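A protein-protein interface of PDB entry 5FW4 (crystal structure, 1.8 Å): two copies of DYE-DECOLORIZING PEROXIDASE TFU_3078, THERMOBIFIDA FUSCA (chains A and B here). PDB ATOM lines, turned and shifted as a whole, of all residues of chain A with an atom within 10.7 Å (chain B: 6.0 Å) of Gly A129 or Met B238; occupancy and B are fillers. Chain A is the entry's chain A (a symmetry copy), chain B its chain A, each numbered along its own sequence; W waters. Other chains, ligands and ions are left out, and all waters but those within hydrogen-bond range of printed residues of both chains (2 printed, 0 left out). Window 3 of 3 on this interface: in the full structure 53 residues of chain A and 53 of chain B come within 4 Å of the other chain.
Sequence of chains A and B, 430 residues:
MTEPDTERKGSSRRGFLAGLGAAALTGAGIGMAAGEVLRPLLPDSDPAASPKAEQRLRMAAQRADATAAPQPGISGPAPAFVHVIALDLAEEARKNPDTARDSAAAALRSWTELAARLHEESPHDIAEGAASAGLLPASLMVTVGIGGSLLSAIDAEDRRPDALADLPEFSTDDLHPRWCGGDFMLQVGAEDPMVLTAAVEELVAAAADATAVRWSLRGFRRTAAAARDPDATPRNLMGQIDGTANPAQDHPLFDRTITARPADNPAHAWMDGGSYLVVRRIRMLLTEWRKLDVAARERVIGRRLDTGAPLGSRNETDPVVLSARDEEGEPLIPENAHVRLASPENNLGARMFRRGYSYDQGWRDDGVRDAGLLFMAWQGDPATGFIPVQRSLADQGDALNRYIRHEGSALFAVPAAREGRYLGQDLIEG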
ATOM      1  N   SER A 122     -23.851  -7.850  -0.235  1.00  0.00           N
ATOM      2  CA  SER A 122     -23.926  -7.126  -1.489  1.00  0.00           C
ATOM      3  C   SER A 122     -24.406  -5.706  -1.247  1.00  0.00           C
ATOM      4  O   SER A 122     -25.039  -5.410  -0.194  1.00  0.00           O
ATOM      5  CB  SER A 122     -24.851  -7.850  -2.493  1.00  0.00           C
ATOM      6  OG  SER A 122     -24.513  -9.218  -2.610  1.00  0.00           O
ATOM      7  N   PRO A 123     -24.137  -4.811  -2.204  1.00  0.00           N
ATOM      8  CA  PRO A 123     -24.572  -3.427  -1.998  1.00  0.00           C
ATOM      9  C   PRO A 123     -26.034  -3.308  -1.632  1.00  0.00           C
ATOM     10  O   PRO A 123     -26.369  -2.453  -0.846  1.00  0.00           O
ATOM     11  CB  PRO A 123     -24.312  -2.766  -3.344  1.00  0.00           C
ATOM     12  CG  PRO A 123     -23.196  -3.579  -3.956  1.00  0.00           C
ATOM     13  CD  PRO A 123     -23.472  -4.997  -3.522  1.00  0.00           C
ATOM     14  N   HIS A 124     -26.889  -4.153  -2.212  1.00  0.00           N
ATOM     15  CA  HIS A 124     -28.331  -4.059  -1.988  1.00  0.00           C
ATOM     16  C   HIS A 124     -28.746  -4.650  -0.642  1.00  0.00           C
ATOM     17  O   HIS A 124     -29.879  -4.423  -0.202  1.00  0.00           O
ATOM     18  CB  HIS A 124     -29.151  -4.681  -3.132  1.00  0.00           C
ATOM     19  CG  HIS A 124     -28.623  -5.986  -3.633  1.00  0.00           C
ATOM     20  ND1 HIS A 124     -27.494  -6.085  -4.428  1.00  0.00           N
ATOM     21  CD2 HIS A 124     -29.090  -7.250  -3.484  1.00  0.00           C
ATOM     22  CE1 HIS A 124     -27.284  -7.353  -4.732  1.00  0.00           C
ATOM     23  NE2 HIS A 124     -28.241  -8.080  -4.181  1.00  0.00           N
ATOM     24  N   ASP A 125     -27.844  -5.379   0.020  1.00  0.00           N
ATOM     25  CA  ASP A 125     -28.051  -5.740   1.448  1.00  0.00           C
ATOM     26  C   ASP A 125     -27.705  -4.559   2.377  1.00  0.00           C
ATOM     27  O   ASP A 125     -28.277  -4.401   3.463  1.00  0.00           O
ATOM     28  CB  ASP A 125     -27.210  -6.970   1.823  1.00  0.00           C
ATOM     29  CG  ASP A 125     -27.485  -8.169   0.926  1.00  0.00           C
ATOM     30  OD1 ASP A 125     -28.664  -8.392   0.579  1.00  0.00           O
ATOM     31  OD2 ASP A 125     -26.521  -8.886   0.560  1.00  0.00           O
ATOM     32  N   ILE A 126     -26.778  -3.718   1.937  1.00  0.00           N
ATOM     33  CA  ILE A 126     -26.312  -2.568   2.730  1.00  0.00           C
ATOM     34  C   ILE A 126     -27.272  -1.376   2.721  1.00  0.00           C
ATOM     35  O   ILE A 126     -27.301  -0.568   3.664  1.00  0.00           O
ATOM     36  CB  ILE A 126     -24.908  -2.146   2.228  1.00  0.00           C
ATOM     37  CG1 ILE A 126     -23.884  -3.138   2.778  1.00  0.00           C
ATOM     38  CG2 ILE A 126     -24.534  -0.704   2.597  1.00  0.00           C
ATOM     39  CD1 ILE A 126     -22.682  -3.293   1.893  1.00  0.00           C
ATOM     40  N   ALA A 127     -28.047  -1.256   1.656  1.00  0.00           N
ATOM     41  CA  ALA A 127     -28.902  -0.100   1.476  1.00  0.00           C
ATOM     42  C   ALA A 127     -30.064  -0.458   0.590  1.00  0.00           C
ATOM     43  O   ALA A 127     -29.902  -1.222  -0.361  1.00  0.00           O
ATOM     44  CB  ALA A 127     -28.108   1.033   0.850  1.00  0.00           C
ATOM     45  N   GLU A 128     -31.227   0.093   0.905  1.00  0.00           N
ATOM     46  CA  GLU A 128     -32.409  -0.039   0.063  1.00  0.00           C
ATOM     47  C   GLU A 128     -32.203   0.712  -1.242  1.00  0.00           C
ATOM     48  O   GLU A 128     -31.461   1.691  -1.304  1.00  0.00           O
ATOM     49  CB  GLU A 128     -33.660   0.541   0.764  1.00  0.00           C
ATOM     50  CG  GLU A 128     -34.319  -0.309   1.836  1.00  0.00           C
ATOM     51  CD  GLU A 128     -35.421   0.441   2.633  1.00  0.00           C
ATOM     52  OE1 GLU A 128     -35.100   1.223   3.562  1.00  0.00           O
ATOM     53  OE2 GLU A 128     -36.629   0.224   2.369  1.00  0.00           O
ATOM     54  N   GLY A 129     -32.885   0.266  -2.288  1.00  0.00           N
ATOM     55  CA  GLY A 129     -32.947   1.014  -3.531  1.00  0.00           C
ATOM     56  C   GLY A 129     -31.637   0.987  -4.329  1.00  0.00           C
ATOM     57  O   GLY A 129     -31.441   1.821  -5.167  1.00  0.00           O
ATOM     58  N   ALA A 130     -30.742   0.064  -4.035  1.00  0.00           N
ATOM     59  CA  ALA A 130     -29.484  -0.010  -4.822  1.00  0.00           C
ATOM     60  C   ALA A 130     -29.697  -0.564  -6.203  1.00  0.00           C
ATOM     61  O   ALA A 130     -30.643  -1.299  -6.472  1.00  0.00           O
ATOM     62  CB  ALA A 130     -28.411  -0.802  -4.078  1.00  0.00           C
ATOM     63  N   ALA A 131     -28.752  -0.242  -7.094  1.00  0.00           N
ATOM     64  CA  ALA A 131     -28.906  -0.553  -8.506  1.00  0.00           C
ATOM     65  C   ALA A 131     -28.766  -2.047  -8.719  1.00  0.00           C
ATOM     66  O   ALA A 131     -29.257  -2.596  -9.696  1.00  0.00           O
ATOM     67  CB  ALA A 131     -27.913   0.238  -9.315  1.00  0.00           C
ATOM     68  N   SER A 132     -28.144  -2.699  -7.758  1.00  0.00           N
ATOM     69  CA  SER A 132     -27.810  -4.121  -7.846  1.00  0.00           C
ATOM     70  C   SER A 132     -28.816  -5.060  -7.239  1.00  0.00           C
ATOM     71  O   SER A 132     -28.573  -6.280  -7.140  1.00  0.00           O
ATOM     72  CB  SER A 132     -26.425  -4.338  -7.208  1.00  0.00           C
ATOM     73  OG  SER A 132     -26.399  -3.921  -5.869  1.00  0.00           O
ATOM     74  N   ALA A 133     -29.959  -4.524  -6.753  1.00  0.00           N
ATOM     75  CA  ALA A 133     -30.928  -5.407  -6.165  1.00  0.00           C
ATOM     76  C   ALA A 133     -31.300  -6.506  -7.179  1.00  0.00           C
ATOM     77  O   ALA A 133     -31.540  -6.228  -8.352  1.00  0.00           O
ATOM     78  CB  ALA A 133     -32.176  -4.647  -5.692  1.00  0.00           C
ATOM     79  N   GLY A 134     -31.385  -7.735  -6.668  1.00  0.00           N
ATOM     80  CA  GLY A 134     -31.874  -8.876  -7.396  1.00  0.00           C
ATOM     81  C   GLY A 134     -30.676  -9.556  -8.082  1.00  0.00           C
ATOM     82  O   GLY A 134     -30.863 -10.487  -8.849  1.00  0.00           O
ATOM     83  N   MET A 194     -23.123  -3.953 -12.959  1.00  0.00           N
ATOM     84  CA  MET A 194     -24.149  -3.302 -12.123  1.00  0.00           C
ATOM     85  C   MET A 194     -23.871  -3.442 -10.631  1.00  0.00           C
ATOM     86  O   MET A 194     -24.080  -2.473  -9.817  1.00  0.00           O
ATOM     87  CB  MET A 194     -25.523  -3.878 -12.466  1.00  0.00           C
ATOM     88  CG  MET A 194     -26.639  -3.001 -11.961  1.00  0.00           C
ATOM     89  SD  MET A 194     -26.656  -1.333 -12.654  1.00  0.00           S
ATOM     90  CE  MET A 194     -27.455  -1.364 -14.230  1.00  0.00           C
ATOM     91  N   THR A 197     -20.969  -0.886 -10.029  1.00  0.00           N
ATOM     92  CA  THR A 197     -21.218   0.545  -9.975  1.00  0.00           C
ATOM     93  C   THR A 197     -22.024   0.815  -8.650  1.00  0.00           C
ATOM     94  O   THR A 197     -21.894   1.857  -8.105  1.00  0.00           O
ATOM     95  CB  THR A 197     -22.008   1.045 -11.199  1.00  0.00           C
ATOM     96  OG1 THR A 197     -22.089   2.498 -11.253  1.00  0.00           O
ATOM     97  CG2 THR A 197     -23.413   0.486 -11.251  1.00  0.00           C
ATOM     98  N   ALA A 198     -22.726  -0.176  -8.147  1.00  0.00           N
ATOM     99  CA  ALA A 198     -23.548   0.016  -6.874  1.00  0.00           C
ATOM    100  C   ALA A 198     -22.611   0.120  -5.690  1.00  0.00           C
ATOM    101  O   ALA A 198     -22.782   0.924  -4.766  1.00  0.00           O
ATOM    102  CB  ALA A 198     -24.455  -1.168  -6.702  1.00  0.00           C
ATOM    103  N   ALA A 199     -21.585  -0.715  -5.724  1.00  0.00           N
ATOM    104  CA  ALA A 199     -20.570  -0.728  -4.698  1.00  0.00           C
ATOM    105  C   ALA A 199     -19.727   0.512  -4.763  1.00  0.00           C
ATOM    106  O   ALA A 199     -19.404   1.060  -3.738  1.00  0.00           O
ATOM    107  CB  ALA A 199     -19.690  -1.969  -4.845  1.00  0.00           C
ATOM    108  N   GLU A 201     -20.624   3.483  -5.874  1.00  0.00           N
ATOM    109  CA  GLU A 201     -21.457   4.598  -5.290  1.00  0.00           C
ATOM    110  C   GLU A 201     -21.388   4.657  -3.780  1.00  0.00           C
ATOM    111  O   GLU A 201     -21.337   5.756  -3.191  1.00  0.00           O
ATOM    112  CB  GLU A 201     -22.905   4.447  -5.692  1.00  0.00           C
ATOM    113  CG  GLU A 201     -23.199   4.713  -7.132  1.00  0.00           C
ATOM    114  CD  GLU A 201     -22.839   6.121  -7.591  1.00  0.00           C
ATOM    115  OE1 GLU A 201     -22.950   7.076  -6.802  1.00  0.00           O
ATOM    116  OE2 GLU A 201     -22.425   6.266  -8.748  1.00  0.00           O
ATOM    117  N   GLU A 202     -21.447   3.501  -3.140  1.00  0.00           N
ATOM    118  CA  GLU A 202     -21.426   3.448  -1.652  1.00  0.00           C
ATOM    119  C   GLU A 202     -20.038   3.762  -1.109  1.00  0.00           C
ATOM    120  O   GLU A 202     -19.871   4.424  -0.139  1.00  0.00           O
ATOM    121  CB  GLU A 202     -21.849   2.073  -1.146  1.00  0.00           C
ATOM    122  CG  GLU A 202     -23.221   1.617  -1.563  1.00  0.00           C
ATOM    123  CD  GLU A 202     -24.327   2.479  -0.981  1.00  0.00           C
ATOM    124  OE1 GLU A 202     -24.257   2.837   0.191  1.00  0.00           O
ATOM    125  OE2 GLU A 202     -25.246   2.828  -1.743  1.00  0.00           O
ATOM    126  N   ASN B 236     -32.085   0.397 -13.272  1.00  0.00           N
ATOM    127  CA  ASN B 236     -31.209   1.524 -13.647  1.00  0.00           C
ATOM    128  C   ASN B 236     -30.329   1.979 -12.494  1.00  0.00           C
ATOM    129  O   ASN B 236     -30.312   1.282 -11.434  1.00  0.00           O
ATOM    130  CB  ASN B 236     -31.968   2.637 -14.317  1.00  0.00           C
ATOM    131  CG  ASN B 236     -32.982   3.274 -13.357  1.00  0.00           C
ATOM    132  OD1 ASN B 236     -32.744   3.212 -12.180  1.00  0.00           O
ATOM    133  ND2 ASN B 236     -33.996   3.895 -13.869  1.00  0.00           N
ATOM    134  N   LEU B 237     -29.566   3.069 -12.660  1.00  0.00           N
ATOM    135  CA  LEU B 237     -28.566   3.420 -11.661  1.00  0.00           C
ATOM    136  C   LEU B 237     -29.311   4.101 -10.493  1.00  0.00           C
ATOM    137  O   LEU B 237     -28.775   4.257  -9.443  1.00  0.00           O
ATOM    138  CB  LEU B 237     -27.569   4.385 -12.133  1.00  0.00           C
ATOM    139  CG  LEU B 237     -26.694   3.690 -13.266  1.00  0.00           C
ATOM    140  CD1 LEU B 237     -25.636   4.692 -13.604  1.00  0.00           C
ATOM    141  CD2 LEU B 237     -26.100   2.417 -12.715  1.00  0.00           C
ATOM    142  N   MET B 238     -30.500   4.501 -10.774  1.00  0.00           N
ATOM    143  CA  MET B 238     -31.378   5.027  -9.645  1.00  0.00           C
ATOM    144  C   MET B 238     -32.064   3.911  -8.848  1.00  0.00           C
ATOM    145  O   MET B 238     -32.918   4.195  -7.965  1.00  0.00           O
ATOM    146  CB  MET B 238     -32.359   5.971 -10.298  1.00  0.00           C
ATOM    147  CG  MET B 238     -31.941   7.413 -10.297  1.00  0.00           C
ATOM    148  SD  MET B 238     -33.028   8.454 -11.246  1.00  0.00           S
ATOM    149  CE  MET B 238     -32.199   9.989 -11.151  1.00  0.00           C
ATOM    150  N   GLY B 239     -31.734   2.648  -9.093  1.00  0.00           N
ATOM    151  CA  GLY B 239     -32.339   1.510  -8.440  1.00  0.00           C
ATOM    152  C   GLY B 239     -33.693   1.049  -8.924  1.00  0.00           C
ATOM    153  O   GLY B 239     -34.259   0.104  -8.387  1.00  0.00           O
ATOM    154  N   GLN B 240     -34.207   1.697  -9.958  1.00  0.00           N
ATOM    155  CA  GLN B 240     -35.588   1.476 -10.370  1.00  0.00           C
ATOM    156  C   GLN B 240     -35.674   0.353 -11.355  1.00  0.00           C
ATOM    157  O   GLN B 240     -34.774   0.203 -12.194  1.00  0.00           O
ATOM    158  CB  GLN B 240     -36.164   2.751 -11.040  1.00  0.00           C
ATOM    159  CG  GLN B 240     -36.104   4.004 -10.142  1.00  0.00           C
ATOM    160  CD  GLN B 240     -35.815   5.307 -10.852  1.00  0.00           C
ATOM    161  OE1 GLN B 240     -35.444   5.361 -12.047  1.00  0.00           O
ATOM    162  NE2 GLN B 240     -35.948   6.395 -10.111  1.00  0.00           N
ATOM    163  N   MET B 284     -27.664  11.370 -14.553  1.00  0.00           N
ATOM    164  CA  MET B 284     -28.399  11.248 -13.252  1.00  0.00           C
ATOM    165  C   MET B 284     -27.666  11.996 -12.153  1.00  0.00           C
ATOM    166  O   MET B 284     -26.466  11.844 -11.969  1.00  0.00           O
ATOM    167  CB  MET B 284     -28.548   9.780 -12.882  1.00  0.00           C
ATOM    168  CG  MET B 284     -29.491   9.032 -13.786  1.00  0.00           C
ATOM    169  SD  MET B 284     -29.501   7.341 -13.415  1.00  0.00           S
ATOM    170  CE  MET B 284     -30.861   6.708 -14.269  1.00  0.00           C
ATOM    171  N   LEU B 285     -28.384  12.817 -11.364  1.00  0.00           N
ATOM    172  CA  LEU B 285     -27.762  13.507 -10.231  1.00  0.00           C
ATOM    173  C   LEU B 285     -27.809  12.586  -9.018  1.00  0.00           C
ATOM    174  O   LEU B 285     -28.684  12.712  -8.126  1.00  0.00           O
ATOM    175  CB  LEU B 285     -28.494  14.847  -9.904  1.00  0.00           C
ATOM    176  CG  LEU B 285     -28.024  16.095 -10.681  1.00  0.00           C
ATOM    177  CD1 LEU B 285     -28.047  15.867 -12.192  1.00  0.00           C
ATOM    178  CD2 LEU B 285     -28.783  17.380 -10.308  1.00  0.00           C
ATOM    179  N   LEU B 286     -26.887  11.646  -8.966  1.00  0.00           N
ATOM    180  CA  LEU B 286     -27.036  10.545  -8.034  1.00  0.00           C
ATOM    181  C   LEU B 286     -26.775  10.951  -6.605  1.00  0.00           C
ATOM    182  O   LEU B 286     -27.402  10.414  -5.681  1.00  0.00           O
ATOM    183  CB  LEU B 286     -26.150   9.359  -8.443  1.00  0.00           C
ATOM    184  CG  LEU B 286     -26.563   8.676  -9.733  1.00  0.00           C
ATOM    185  CD1 LEU B 286     -25.498   7.644 -10.142  1.00  0.00           C
ATOM    186  CD2 LEU B 286     -27.937   8.005  -9.691  1.00  0.00           C
ATOM    187  N   TRP B 289     -30.007  12.536  -5.587  1.00  0.00           N
ATOM    188  CA  TRP B 289     -30.941  11.412  -5.521  1.00  0.00           C
ATOM    189  C   TRP B 289     -30.720  10.575  -4.270  1.00  0.00           C
ATOM    190  O   TRP B 289     -31.683  10.142  -3.670  1.00  0.00           O
ATOM    191  CB  TRP B 289     -30.789  10.511  -6.758  1.00  0.00           C
ATOM    192  CG  TRP B 289     -31.665   9.325  -6.806  1.00  0.00           C
ATOM    193  CD1 TRP B 289     -31.303   8.037  -6.553  1.00  0.00           C
ATOM    194  CD2 TRP B 289     -33.073   9.288  -7.109  1.00  0.00           C
ATOM    195  NE1 TRP B 289     -32.356   7.206  -6.728  1.00  0.00           N
ATOM    196  CE2 TRP B 289     -33.468   7.943  -7.047  1.00  0.00           C
ATOM    197  CE3 TRP B 289     -34.026  10.258  -7.459  1.00  0.00           C
ATOM    198  CZ2 TRP B 289     -34.771   7.540  -7.326  1.00  0.00           C
ATOM    199  CZ3 TRP B 289     -35.289   9.846  -7.779  1.00  0.00           C
ATOM    200  CH2 TRP B 289     -35.659   8.511  -7.694  1.00  0.00           C
ATOM    201  N   VAL B 294     -36.399   6.381   0.745  1.00  0.00           N
ATOM    202  CA  VAL B 294     -36.948   5.443  -0.246  1.00  0.00           C
ATOM    203  C   VAL B 294     -38.342   5.871  -0.642  1.00  0.00           C
ATOM    204  O   VAL B 294     -38.664   5.937  -1.804  1.00  0.00           O
ATOM    205  CB  VAL B 294     -36.911   3.982   0.292  1.00  0.00           C
ATOM    206  CG1 VAL B 294     -37.875   3.058  -0.455  1.00  0.00           C
ATOM    207  CG2 VAL B 294     -35.486   3.422   0.226  1.00  0.00           C
ATOM    208  N   ARG B 297     -38.250   8.738  -3.114  1.00  0.00           N
ATOM    209  CA  ARG B 297     -37.790   8.264  -4.452  1.00  0.00           C
ATOM    210  C   ARG B 297     -38.939   7.627  -5.218  1.00  0.00           C
ATOM    211  O   ARG B 297     -39.201   7.930  -6.380  1.00  0.00           O
ATOM    212  CB  ARG B 297     -36.686   7.248  -4.272  1.00  0.00           C
ATOM    213  CG  ARG B 297     -35.401   7.818  -3.680  1.00  0.00           C
ATOM    214  CD  ARG B 297     -34.458   6.676  -3.286  1.00  0.00           C
ATOM    215  NE  ARG B 297     -33.309   7.126  -2.518  1.00  0.00           N
ATOM    216  CZ  ARG B 297     -32.161   6.455  -2.378  1.00  0.00           C
ATOM    217  NH1 ARG B 297     -31.971   5.249  -2.912  1.00  0.00           N
ATOM    218  NH2 ARG B 297     -31.179   7.002  -1.669  1.00  0.00           N
ATOM    219  N   LEU B 305     -39.611   0.849  -5.395  1.00  0.00           N
ATOM    220  CA  LEU B 305     -38.278   0.334  -5.787  1.00  0.00           C
ATOM    221  C   LEU B 305     -38.130  -1.179  -5.626  1.00  0.00           C
ATOM    222  O   LEU B 305     -37.472  -1.838  -6.450  1.00  0.00           O
ATOM    223  CB  LEU B 305     -37.180   1.037  -4.984  1.00  0.00           C
ATOM    224  CG  LEU B 305     -36.952   2.519  -5.292  1.00  0.00           C
ATOM    225  CD1 LEU B 305     -36.169   3.193  -4.177  1.00  0.00           C
ATOM    226  CD2 LEU B 305     -36.225   2.707  -6.619  1.00  0.00           C
ATOM    227  N   LEU B 400     -39.120  13.981 -11.758  1.00  0.00           N
ATOM    228  CA  LEU B 400     -37.794  13.462 -12.118  1.00  0.00           C
ATOM    229  C   LEU B 400     -36.818  14.498 -12.698  1.00  0.00           C
ATOM    230  O   LEU B 400     -35.578  14.315 -12.583  1.00  0.00           O
ATOM    231  CB  LEU B 400     -37.991  12.324 -13.094  1.00  0.00           C
ATOM    232  CG  LEU B 400     -36.758  11.550 -13.617  1.00  0.00           C
ATOM    233  CD1 LEU B 400     -35.991  10.900 -12.484  1.00  0.00           C
ATOM    234  CD2 LEU B 400     -37.294  10.491 -14.558  1.00  0.00           C
ATOM    235  N   TYR B 403     -33.591  15.582 -11.077  1.00  0.00           N
ATOM    236  CA  TYR B 403     -32.510  14.644 -10.821  1.00  0.00           C
ATOM    237  C   TYR B 403     -31.825  14.186 -12.103  1.00  0.00           C
ATOM    238  O   TYR B 403     -31.030  13.269 -12.033  1.00  0.00           O
ATOM    239  CB  TYR B 403     -33.008  13.430 -10.083  1.00  0.00           C
ATOM    240  CG  TYR B 403     -33.560  13.848  -8.705  1.00  0.00           C
ATOM    241  CD1 TYR B 403     -32.708  14.151  -7.665  1.00  0.00           C
ATOM    242  CD2 TYR B 403     -34.902  13.996  -8.512  1.00  0.00           C
ATOM    243  CE1 TYR B 403     -33.211  14.613  -6.396  1.00  0.00           C
ATOM    244  CE2 TYR B 403     -35.406  14.422  -7.275  1.00  0.00           C
ATOM    245  CZ  TYR B 403     -34.534  14.722  -6.236  1.00  0.00           C
ATOM    246  OH  TYR B 403     -35.052  15.165  -4.974  1.00  0.00           O
ATOM    247  N   ILE B 404     -32.227  14.761 -13.214  1.00  0.00           N
ATOM    248  CA  ILE B 404     -31.668  14.384 -14.527  1.00  0.00           C
ATOM    249  C   ILE B 404     -31.334  15.575 -15.402  1.00  0.00           C
ATOM    250  O   ILE B 404     -31.953  16.626 -15.286  1.00  0.00           O
ATOM    251  CB  ILE B 404     -32.624  13.473 -15.340  1.00  0.00           C
ATOM    252  CG1 ILE B 404     -33.841  14.262 -15.861  1.00  0.00           C
ATOM    253  CG2 ILE B 404     -32.940  12.208 -14.577  1.00  0.00           C
ATOM    254  CD1 ILE B 404     -34.913  13.441 -16.542  1.00  0.00           C
HETATM  255  O   HOH W   1     -32.912   4.037  -5.197  1.00  0.00           O
HETATM  256  O   HOH W   2     -33.314  -1.191  -5.922  1.00  0.00           O
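Among the printed residues, merely in contact across the chains: Glu A128 with Val B294 (3.5 Å), Glu A128 with Arg B297 (3.9 Å), Gly A129 with Met B238 (3.96 Å), Gly A129 with Gly B239 (3.4 Å), Gly A129 with Leu B305 (3.9 Å), Ala A130 with Gly B239 (3.8 Å), Ala A131 with Asn B236 (3.4 Å), Met A194 with Leu B237 (3.8 Å), Thr A197 with Leu B237 (3.6 Å) and Glu A201 with Leu B286 (3.6 Å).
Water W1 lies within hydrogen-bond range of the backbone carbonyl oxygen of Gly A129, the guanidinium group of Arg B297 and the backbone carbonyl oxygen of Met B238. Water W2 lies within hydrogen-bond range of the backbone carbonyl oxygen of Ala A130 (2.7 Å) and the backbone carbonyl oxygen of Gly B239 (2.9 Å).
Of the 19 printed residues of chain A, 7 touch a printed residue of chain B. Printed residues of chain A that touch a printed residue of chain B: Glu A128, Gly A129, Ala A130, Ala A131, Met A194, Thr A197 and Glu A201. Hydrophobic or aromatic side chains of chain A within 4 Å of the printed part of chain B: Ala A131 and Met A194. Of the 15 printed residues of chain B, 8 touch a printed residue of chain A. Hydrophobic or aromatic side chains of chain B that line the printed part of chain A: Leu B237, Leu B286, Val B294 and Leu B305. Among the printed residues, no Asp or Glu carboxylate lies within 4 Å of a Lys or Arg side-chain nitrogen of the other chain.
The side-chain amide oxygen of Asn B236 is in hydrogen-bond range of the backbone NH of Met B238, at 2.9 Å. The side-chain amide oxygen (OD1) of Asn B236 sits at hydrogen-bond distance from the backbone NH (N) of Gly B239 (3.3 Å). The side-chain amide nitrogen of Asn B236 lies within hydrogen-bond range of the side-chain amide oxygen of Gln B240. The side-chain amide nitrogen (NE2) of Gln B240 lies close to the side-chain sulfur (SD) of Met B238 (3.7 Å). O of Met B238 is in hydrogen-bond range of NE1 of Trp B289.
No position is printed for both chains.
Gly A129 touches just these residues of chain B: Met B238 (3.96 Å), Gly B239 (3.4 Å) and Leu B305 (3.9 Å). Of chain A, only Ala A131 (3.4 Å) comes within 4 Å of Asn B236. Met B238 touches just one residue of chain A: Gly A129. No residue of chain A comes within 4 Å of Gln B240. No residue of chain A comes within 4 Å of Met B284. Printed residues of chain A within 4 Å of Val B294: Glu A128 (3.5 Å). Of the printed residues of chain A, Arg B297 touches Glu A128. The nearest residue of chain A that does not touch Met B238 is Ala A131 (5.2 Å). The nearest printed residue of chain B that does not touch Thr A197 is Leu B286 (6.3 Å).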
